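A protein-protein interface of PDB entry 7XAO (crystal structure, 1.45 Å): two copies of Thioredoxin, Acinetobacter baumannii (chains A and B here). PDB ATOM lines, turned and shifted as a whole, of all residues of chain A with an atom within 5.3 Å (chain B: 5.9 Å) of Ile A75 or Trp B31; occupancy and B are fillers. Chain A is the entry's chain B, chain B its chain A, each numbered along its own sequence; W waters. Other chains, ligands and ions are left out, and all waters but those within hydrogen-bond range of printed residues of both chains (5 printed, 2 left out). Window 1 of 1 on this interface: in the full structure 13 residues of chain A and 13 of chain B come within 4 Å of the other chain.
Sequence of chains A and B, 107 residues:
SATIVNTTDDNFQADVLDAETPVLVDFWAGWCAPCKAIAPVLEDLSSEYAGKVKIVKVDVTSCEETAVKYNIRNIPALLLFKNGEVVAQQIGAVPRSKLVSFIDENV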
ATOM      1  N   PHE A  27      -7.254 -23.937  31.107  1.00  0.00           N
ATOM      2  CA  PHE A  27      -6.037 -24.743  31.075  1.00  0.00           C
ATOM      3  C   PHE A  27      -4.936 -24.009  31.843  1.00  0.00           C
ATOM      4  O   PHE A  27      -4.585 -22.878  31.480  1.00  0.00           O
ATOM      5  CB  PHE A  27      -5.624 -24.964  29.620  1.00  0.00           C
ATOM      6  CG  PHE A  27      -6.559 -25.845  28.832  1.00  0.00           C
ATOM      7  CD1 PHE A  27      -7.680 -25.306  28.235  1.00  0.00           C
ATOM      8  CD2 PHE A  27      -6.285 -27.197  28.661  1.00  0.00           C
ATOM      9  CE1 PHE A  27      -8.539 -26.096  27.497  1.00  0.00           C
ATOM     10  CE2 PHE A  27      -7.132 -27.995  27.926  1.00  0.00           C
ATOM     11  CZ  PHE A  27      -8.255 -27.451  27.334  1.00  0.00           C
ATOM     12  N   TRP A  28      -4.410 -24.640  32.904  1.00  0.00           N
ATOM     13  CA  TRP A  28      -3.516 -23.979  33.849  1.00  0.00           C
ATOM     14  C   TRP A  28      -2.418 -24.944  34.292  1.00  0.00           C
ATOM     15  O   TRP A  28      -2.477 -26.148  34.015  1.00  0.00           O
ATOM     16  CB  TRP A  28      -4.301 -23.471  35.082  1.00  0.00           C
ATOM     17  CG  TRP A  28      -4.706 -24.579  36.001  1.00  0.00           C
ATOM     18  CD1 TRP A  28      -5.713 -25.486  35.799  1.00  0.00           C
ATOM     19  CD2 TRP A  28      -4.093 -24.934  37.240  1.00  0.00           C
ATOM     20  NE1 TRP A  28      -5.774 -26.360  36.846  1.00  0.00           N
ATOM     21  CE2 TRP A  28      -4.785 -26.054  37.743  1.00  0.00           C
ATOM     22  CE3 TRP A  28      -3.036 -24.400  37.986  1.00  0.00           C
ATOM     23  CZ2 TRP A  28      -4.451 -26.656  38.952  1.00  0.00           C
ATOM     24  CZ3 TRP A  28      -2.700 -24.998  39.177  1.00  0.00           C
ATOM     25  CH2 TRP A  28      -3.401 -26.119  39.651  1.00  0.00           C
ATOM     26  N   ALA A  29      -1.415 -24.414  35.001  1.00  0.00           N
ATOM     27  CA  ALA A  29      -0.388 -25.222  35.659  1.00  0.00           C
ATOM     28  C   ALA A  29       0.074 -24.528  36.929  1.00  0.00           C
ATOM     29  O   ALA A  29       0.053 -23.301  37.017  1.00  0.00           O
ATOM     30  CB  ALA A  29       0.831 -25.467  34.758  1.00  0.00           C
ATOM     31  N   TRP A  31       3.048 -23.968  38.204  1.00  0.00           N
ATOM     32  CA  TRP A  31       4.154 -23.027  38.063  1.00  0.00           C
ATOM     33  C   TRP A  31       3.771 -21.762  37.315  1.00  0.00           C
ATOM     34  O   TRP A  31       4.552 -20.803  37.311  1.00  0.00           O
ATOM     35  CB  TRP A  31       5.330 -23.679  37.325  1.00  0.00           C
ATOM     36  CG  TRP A  31       4.954 -24.306  36.017  1.00  0.00           C
ATOM     37  CD1 TRP A  31       4.684 -25.628  35.793  1.00  0.00           C
ATOM     38  CD2 TRP A  31       4.801 -23.648  34.750  1.00  0.00           C
ATOM     39  NE1 TRP A  31       4.362 -25.831  34.473  1.00  0.00           N
ATOM     40  CE2 TRP A  31       4.432 -24.632  33.812  1.00  0.00           C
ATOM     41  CE3 TRP A  31       4.940 -22.319  34.316  1.00  0.00           C
ATOM     42  CZ2 TRP A  31       4.185 -24.334  32.476  1.00  0.00           C
ATOM     43  CZ3 TRP A  31       4.694 -22.026  32.995  1.00  0.00           C
ATOM     44  CH2 TRP A  31       4.311 -23.027  32.088  1.00  0.00           C
ATOM     45  N   CYS A  32       2.619 -21.734  36.655  1.00  0.00           N
ATOM     46  CA  CYS A  32       2.303 -20.668  35.726  1.00  0.00           C
ATOM     47  C   CYS A  32       1.759 -19.446  36.460  1.00  0.00           C
ATOM     48  O   CYS A  32       0.735 -19.517  37.160  1.00  0.00           O
ATOM     49  CB  CYS A  32       1.337 -21.198  34.679  1.00  0.00           C
ATOM     50  N   PRO A  34       0.601 -16.235  35.256  1.00  0.00           N
ATOM     51  CA  PRO A  34      -0.676 -15.614  34.849  1.00  0.00           C
ATOM     52  C   PRO A  34      -1.866 -16.469  35.210  1.00  0.00           C
ATOM     53  O   PRO A  34      -2.967 -15.950  35.390  1.00  0.00           O
ATOM     54  CB  PRO A  34      -0.545 -15.452  33.327  1.00  0.00           C
ATOM     55  CG  PRO A  34       0.912 -15.563  33.051  1.00  0.00           C
ATOM     56  CD  PRO A  34       1.507 -16.437  34.112  1.00  0.00           C
ATOM     57  N   CYS A  35      -1.679 -17.779  35.310  1.00  0.00           N
ATOM     58  CA  CYS A  35      -2.756 -18.642  35.773  1.00  0.00           C
ATOM     59  C   CYS A  35      -3.180 -18.243  37.178  1.00  0.00           C
ATOM     60  O   CYS A  35      -4.378 -18.224  37.492  1.00  0.00           O
ATOM     61  CB  CYS A  35      -2.304 -20.103  35.747  1.00  0.00           C
ATOM     62  SG  CYS A  35      -1.769 -20.759  34.120  1.00  0.00           S
ATOM     63  N   VAL A  60      -2.637 -28.921  33.126  1.00  0.00           N
ATOM     64  CA  VAL A  60      -1.961 -29.492  31.969  1.00  0.00           C
ATOM     65  C   VAL A  60      -0.819 -30.420  32.345  1.00  0.00           C
ATOM     66  O   VAL A  60      -0.445 -31.272  31.536  1.00  0.00           O
ATOM     67  CB  VAL A  60      -1.508 -28.402  30.994  1.00  0.00           C
ATOM     68  CG1 VAL A  60      -2.714 -27.575  30.608  1.00  0.00           C
ATOM     69  CG2 VAL A  60      -0.432 -27.533  31.654  1.00  0.00           C
ATOM     70  N   GLU A  64      -1.792 -33.563  29.725  1.00  0.00           N
ATOM     71  CA  GLU A  64      -1.107 -33.162  28.502  1.00  0.00           C
ATOM     72  C   GLU A  64      -1.888 -33.576  27.259  1.00  0.00           C
ATOM     73  O   GLU A  64      -1.934 -32.837  26.270  1.00  0.00           O
ATOM     74  CB  GLU A  64       0.291 -33.791  28.477  1.00  0.00           C
ATOM     75  CG  GLU A  64       1.081 -33.501  27.214  1.00  0.00           C
ATOM     76  CD  GLU A  64       2.339 -34.342  27.115  1.00  0.00           C
ATOM     77  OE1 GLU A  64       2.302 -35.534  27.498  1.00  0.00           O
ATOM     78  OE2 GLU A  64       3.362 -33.807  26.647  1.00  0.00           O
ATOM     79  N   ALA A  67      -4.656 -30.980  26.588  1.00  0.00           N
ATOM     80  CA  ALA A  67      -4.076 -29.713  26.168  1.00  0.00           C
ATOM     81  C   ALA A  67      -3.602 -29.779  24.729  1.00  0.00           C
ATOM     82  O   ALA A  67      -3.826 -28.839  23.960  1.00  0.00           O
ATOM     83  CB  ALA A  67      -2.915 -29.341  27.086  1.00  0.00           C
ATOM     84  N   VAL A  68      -2.927 -30.875  24.350  1.00  0.00           N
ATOM     85  CA  VAL A  68      -2.456 -31.018  22.976  1.00  0.00           C
ATOM     86  C   VAL A  68      -3.631 -31.200  22.018  1.00  0.00           C
ATOM     87  O   VAL A  68      -3.648 -30.626  20.924  1.00  0.00           O
ATOM     88  CB  VAL A  68      -1.408 -32.145  22.879  1.00  0.00           C
ATOM     89  CG1 VAL A  68      -1.101 -32.483  21.439  1.00  0.00           C
ATOM     90  CG2 VAL A  68      -0.130 -31.719  23.592  1.00  0.00           C
ATOM     91  N   ILE A  72      -4.125 -25.566  22.522  1.00  0.00           N
ATOM     92  CA  ILE A  72      -4.372 -24.439  23.417  1.00  0.00           C
ATOM     93  C   ILE A  72      -3.375 -23.300  23.270  1.00  0.00           C
ATOM     94  O   ILE A  72      -3.648 -22.217  23.791  1.00  0.00           O
ATOM     95  CB  ILE A  72      -4.449 -24.854  24.903  1.00  0.00           C
ATOM     96  CG1 ILE A  72      -3.122 -25.472  25.370  1.00  0.00           C
ATOM     97  CG2 ILE A  72      -5.662 -25.783  25.172  1.00  0.00           C
ATOM     98  CD1 ILE A  72      -2.957 -25.465  26.892  1.00  0.00           C
ATOM     99  N   ARG A  73      -2.238 -23.514  22.589  1.00  0.00           N
ATOM    100  CA  ARG A  73      -1.213 -22.500  22.289  1.00  0.00           C
ATOM    101  C   ARG A  73      -0.297 -22.138  23.461  1.00  0.00           C
ATOM    102  O   ARG A  73       0.922 -22.136  23.306  1.00  0.00           O
ATOM    103  CB  ARG A  73      -1.792 -21.221  21.668  1.00  0.00           C
ATOM    104  CG  ARG A  73      -2.843 -21.449  20.591  1.00  0.00           C
ATOM    105  CD  ARG A  73      -2.306 -22.329  19.466  1.00  0.00           C
ATOM    106  NE  ARG A  73      -1.523 -21.560  18.494  1.00  0.00           N
ATOM    107  CZ  ARG A  73      -0.797 -22.104  17.524  1.00  0.00           C
ATOM    108  NH1 ARG A  73      -0.752 -23.418  17.369  1.00  0.00           N
ATOM    109  NH2 ARG A  73      -0.116 -21.331  16.698  1.00  0.00           N
ATOM    110  N   ASN A  74      -0.861 -21.757  24.604  1.00  0.00           N
ATOM    111  CA  ASN A  74      -0.110 -21.476  25.821  1.00  0.00           C
ATOM    112  C   ASN A  74      -1.119 -21.423  26.963  1.00  0.00           C
ATOM    113  O   ASN A  74      -2.338 -21.540  26.744  1.00  0.00           O
ATOM    114  CB  ASN A  74       0.704 -20.177  25.696  1.00  0.00           C
ATOM    115  CG  ASN A  74       2.027 -20.229  26.444  1.00  0.00           C
ATOM    116  OD1 ASN A  74       2.143 -20.884  27.468  1.00  0.00           O
ATOM    117  ND2 ASN A  74       3.039 -19.503  25.926  1.00  0.00           N
ATOM    118  N   ILE A  75      -0.604 -21.286  28.182  1.00  0.00           N
ATOM    119  CA  ILE A  75      -1.455 -21.178  29.371  1.00  0.00           C
ATOM    120  C   ILE A  75      -1.282 -19.791  29.984  1.00  0.00           C
ATOM    121  O   ILE A  75      -0.201 -19.185  29.867  1.00  0.00           O
ATOM    122  CB  ILE A  75      -1.183 -22.299  30.390  1.00  0.00           C
ATOM    123  CG1 ILE A  75       0.276 -22.303  30.815  1.00  0.00           C
ATOM    124  CG2 ILE A  75      -1.597 -23.663  29.855  1.00  0.00           C
ATOM    125  CD1 ILE A  75       0.533 -23.333  31.873  1.00  0.00           C
ATOM    126  N   PRO A  76      -2.311 -19.233  30.637  1.00  0.00           N
ATOM    127  CA  PRO A  76      -3.635 -19.855  30.722  1.00  0.00           C
ATOM    128  C   PRO A  76      -4.366 -19.770  29.392  1.00  0.00           C
ATOM    129  O   PRO A  76      -4.220 -18.788  28.672  1.00  0.00           O
ATOM    130  CB  PRO A  76      -4.355 -19.022  31.786  1.00  0.00           C
ATOM    131  CG  PRO A  76      -3.704 -17.698  31.722  1.00  0.00           C
ATOM    132  CD  PRO A  76      -2.261 -17.945  31.350  1.00  0.00           C
ATOM    133  N   ALA A  77      -5.122 -20.815  29.075  1.00  0.00           N
ATOM    134  CA  ALA A  77      -5.972 -20.856  27.895  1.00  0.00           C
ATOM    135  C   ALA A  77      -7.403 -21.036  28.376  1.00  0.00           C
ATOM    136  O   ALA A  77      -7.684 -21.957  29.148  1.00  0.00           O
ATOM    137  CB  ALA A  77      -5.589 -22.013  26.961  1.00  0.00           C
ATOM    138  N   GLY A  92      -4.097 -16.573  27.023  1.00  0.00           N
ATOM    139  CA  GLY A  92      -3.405 -15.600  27.841  1.00  0.00           C
ATOM    140  C   GLY A  92      -4.343 -14.905  28.817  1.00  0.00           C
ATOM    141  O   GLY A  92      -5.560 -14.855  28.639  1.00  0.00           O
ATOM    142  N   ALA B  29       6.850 -27.223  26.347  1.00  0.00           N
ATOM    143  CA  ALA B  29       5.804 -28.225  26.502  1.00  0.00           C
ATOM    144  C   ALA B  29       5.187 -28.486  25.140  1.00  0.00           C
ATOM    145  O   ALA B  29       5.267 -27.654  24.240  1.00  0.00           O
ATOM    146  CB  ALA B  29       4.708 -27.774  27.475  1.00  0.00           C
ATOM    147  N   GLY B  30       4.586 -29.671  24.987  1.00  0.00           N
ATOM    148  CA  GLY B  30       4.031 -30.044  23.689  1.00  0.00           C
ATOM    149  C   GLY B  30       2.843 -29.207  23.250  1.00  0.00           C
ATOM    150  O   GLY B  30       2.612 -29.033  22.049  1.00  0.00           O
ATOM    151  N   TRP B  31       2.088 -28.668  24.206  1.00  0.00           N
ATOM    152  CA  TRP B  31       0.959 -27.781  23.952  1.00  0.00           C
ATOM    153  C   TRP B  31       1.377 -26.327  23.756  1.00  0.00           C
ATOM    154  O   TRP B  31       0.527 -25.478  23.458  1.00  0.00           O
ATOM    155  CB  TRP B  31      -0.049 -27.879  25.108  1.00  0.00           C
ATOM    156  CG  TRP B  31       0.578 -27.805  26.488  1.00  0.00           C
ATOM    157  CD1 TRP B  31       0.773 -28.839  27.371  1.00  0.00           C
ATOM    158  CD2 TRP B  31       1.076 -26.623  27.154  1.00  0.00           C
ATOM    159  NE1 TRP B  31       1.368 -28.374  28.530  1.00  0.00           N
ATOM    160  CE2 TRP B  31       1.561 -27.022  28.419  1.00  0.00           C
ATOM    161  CE3 TRP B  31       1.165 -25.267  26.797  1.00  0.00           C
ATOM    162  CZ2 TRP B  31       2.136 -26.124  29.317  1.00  0.00           C
ATOM    163  CZ3 TRP B  31       1.739 -24.378  27.702  1.00  0.00           C
ATOM    164  CH2 TRP B  31       2.213 -24.809  28.945  1.00  0.00           C
ATOM    165  N   CYS B  32       2.660 -26.022  23.901  1.00  0.00           N
ATOM    166  CA  CYS B  32       3.129 -24.648  23.866  1.00  0.00           C
ATOM    167  C   CYS B  32       3.586 -24.308  22.449  1.00  0.00           C
ATOM    168  O   CYS B  32       4.661 -24.731  22.000  1.00  0.00           O
ATOM    169  CB  CYS B  32       4.223 -24.486  24.912  1.00  0.00           C
ATOM    170  N   ALA B  33       2.765 -23.544  21.743  1.00  0.00           N
ATOM    171  CA  ALA B  33       3.066 -23.267  20.341  1.00  0.00           C
ATOM    172  C   ALA B  33       4.324 -22.425  20.161  1.00  0.00           C
ATOM    173  O   ALA B  33       5.166 -22.789  19.320  1.00  0.00           O
ATOM    174  CB  ALA B  33       1.830 -22.689  19.647  1.00  0.00           C
ATOM    175  N   VAL B  60       8.239 -29.438  30.551  1.00  0.00           N
ATOM    176  CA  VAL B  60       7.640 -29.122  31.854  1.00  0.00           C
ATOM    177  C   VAL B  60       6.483 -30.038  32.242  1.00  0.00           C
ATOM    178  O   VAL B  60       6.083 -30.040  33.407  1.00  0.00           O
ATOM    179  CB  VAL B  60       7.239 -27.635  31.981  1.00  0.00           C
ATOM    180  CG1 VAL B  60       8.449 -26.716  31.720  1.00  0.00           C
ATOM    181  CG2 VAL B  60       6.089 -27.314  31.043  1.00  0.00           C
ATOM    182  N   THR B  61       5.960 -30.837  31.313  1.00  0.00           N
ATOM    183  CA  THR B  61       4.942 -31.823  31.660  1.00  0.00           C
ATOM    184  C   THR B  61       5.486 -32.877  32.620  1.00  0.00           C
ATOM    185  O   THR B  61       4.838 -33.216  33.615  1.00  0.00           O
ATOM    186  CB  THR B  61       4.404 -32.472  30.389  1.00  0.00           C
ATOM    187  OG1 THR B  61       3.729 -31.479  29.616  1.00  0.00           O
ATOM    188  CG2 THR B  61       3.435 -33.633  30.736  1.00  0.00           C
ATOM    189  N   ASN B  74       6.537 -18.492  33.149  1.00  0.00           N
ATOM    190  CA  ASN B  74       5.978 -18.431  31.810  1.00  0.00           C
ATOM    191  C   ASN B  74       6.947 -19.158  30.894  1.00  0.00           C
ATOM    192  O   ASN B  74       8.155 -19.071  31.093  1.00  0.00           O
ATOM    193  CB  ASN B  74       5.882 -16.983  31.309  1.00  0.00           C
ATOM    194  CG  ASN B  74       4.831 -16.176  32.028  1.00  0.00           C
ATOM    195  OD1 ASN B  74       3.648 -16.359  31.790  1.00  0.00           O
ATOM    196  ND2 ASN B  74       5.254 -15.270  32.896  1.00  0.00           N
ATOM    197  N   ILE B  75       6.413 -19.849  29.886  1.00  0.00           N
ATOM    198  CA  ILE B  75       7.228 -20.438  28.819  1.00  0.00           C
ATOM    199  C   ILE B  75       6.793 -19.852  27.480  1.00  0.00           C
ATOM    200  O   ILE B  75       5.631 -19.440  27.355  1.00  0.00           O
ATOM    201  CB  ILE B  75       7.182 -21.979  28.806  1.00  0.00           C
ATOM    202  CG1 ILE B  75       5.763 -22.519  28.510  1.00  0.00           C
ATOM    203  CG2 ILE B  75       7.779 -22.559  30.085  1.00  0.00           C
ATOM    204  CD1 ILE B  75       5.701 -24.032  28.393  1.00  0.00           C
HETATM  205  O   HOH W   1       3.795 -28.632  33.775  1.00  0.00           O
HETATM  206  O   HOH W   2       0.973 -30.896  29.554  1.00  0.00           O
HETATM  207  O   HOH W   3       2.094 -18.991  31.556  1.00  0.00           O
HETATM  208  O   HOH W   4       4.781 -31.668  27.185  1.00  0.00           O
HETATM  209  O   HOH W   5       3.486 -20.059  29.698  1.00  0.00           O
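Of the printed residues of chain B, Ala A67 touches Trp B31.
Of the printed residues of chain B, Val A68 touches Gly B30 (3.9 Å) and Trp B31 (3.8 Å).
Of the printed residues of chain B, Arg A73 touches Trp B31 (3.4 Å), Cys B32 (3.4 Å) and Ala B33 (2.8 Å).
Ala B29 touches none of the printed residues of chain A.
Of chain A, only Val A60 (3.7 Å), Ala A67 (3.7 Å), Val A68 (3.8 Å), Ile A72 (3.9 Å), Arg A73 (3.4 Å), Asn A74 (3.5 Å) and Ile A75 (3.7 Å) come within 4 Å of Trp B31.
Of the printed residues of chain A, Ala B33 touches Arg A73.
Printed residues of chain A within 4 Å of Ile B75: Trp A31 (3.9 Å) and Asn A74 (3.0 Å).
The nearest residue of chain B that does not touch Ile A75 is Asn B74 (5.1 Å).
The nearest residue of chain A that does not touch Trp B31 is Trp A31 (4.1 Å).
The nearest printed residue of chain A that does not touch Ile B75 is Ile A75 (6.0 Å).
Trp A31 touches Val B60, and with the chains exchanged Val A60 touches Trp B31.
Trp A31 touches Asn B74, and with the chains exchanged Asn A74 touches Trp B31.
Trp A31 touches Ile B75, and with the chains exchanged Ile A75 touches Trp B31.
Asn A74 touches Ile B75, but with the chains exchanged Ile A75 does not touch Asn B74 (5.1 Å).
Positions printed for both chains: 29, 31, 32, 60, 74 and 75.
Of the 16 pairs that touch across the chains among the printed residues, 6 have their exchanged pair printed and touching as well.
Water W2 lies within hydrogen-bond range of O of Val A60 (2.5 Å), NE1 of Trp B31 (2.8 Å) and OG1 of Thr B61 (2.8 Å).
Water W4 lies within hydrogen-bond range of the side-chain carboxylate of Glu A64 (2.6 Å), the side-chain hydroxyl of Thr B61 (2.7 Å) and the backbone NH of Gly B30 (3.0 Å).
Water W1 bridges O of Val B60 and NE1 of Trp A31.
Water W5 lies within hydrogen-bond range of the side-chain amide oxygen (OD1) of Asn A74 and the backbone NH (N) of Ile B75.
Water W3 lies within hydrogen-bond range of O of Ile A75 and OD1 of Asn B74.
O of Arg A73 lies close to O of Trp B31 (3.4 Å).
The backbone NH (N) of Ala B33 lies within hydrogen-bond range of the backbone carbonyl oxygen (O) of Arg A73, at 2.8 Å.
The backbone carbonyl oxygen (O) of Ile B75 sits at hydrogen-bond distance from the side-chain amide nitrogen (ND2) of Asn A74 (3.0 Å).
Along chain A the printed residues that touch a printed residue of chain B span positions 31 to 75.
Hydrophobic or aromatic side chains of chain B that line the printed part of chain A: Trp B31, Ala B33, Val B60 and Ile B75.
Along chain B the printed residues that touch a printed residue of chain A span positions 30 to 75.
Among the printed residues, 16 pairs touch across the chains.
Among the printed residues, no Asp or Glu carboxylate lies within 4 Å of a Lys or Arg side-chain nitrogen of the other chain.
Among the printed residues, pairs that only touch across the chains: Trp A31 with Val B60 (3.8 Å), Trp A31 with Asn B74 (3.99 Å), Trp A31 with Ile B75 (3.9 Å), Pro A34 with Asn B74 (3.1 Å), Val A60 with Trp B31 (3.7 Å), Glu A64 with Thr B61 (3.8 Å), Ala A67 with Trp B31 (3.7 Å), Val A68 with Gly B30 (3.9 Å), Val A68 with Trp B31 (3.8 Å), Ile A72 with Trp B31 (3.9 Å), Arg A73 with Cys B32 (3.4 Å), Asn A74 with Trp B31 (3.5 Å) and Ile A75 with Trp B31 (3.7 Å).
The backbone carbonyl oxygen (O) of Trp A28 is in hydrogen-bond range of the backbone NH (N) of Val A60.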
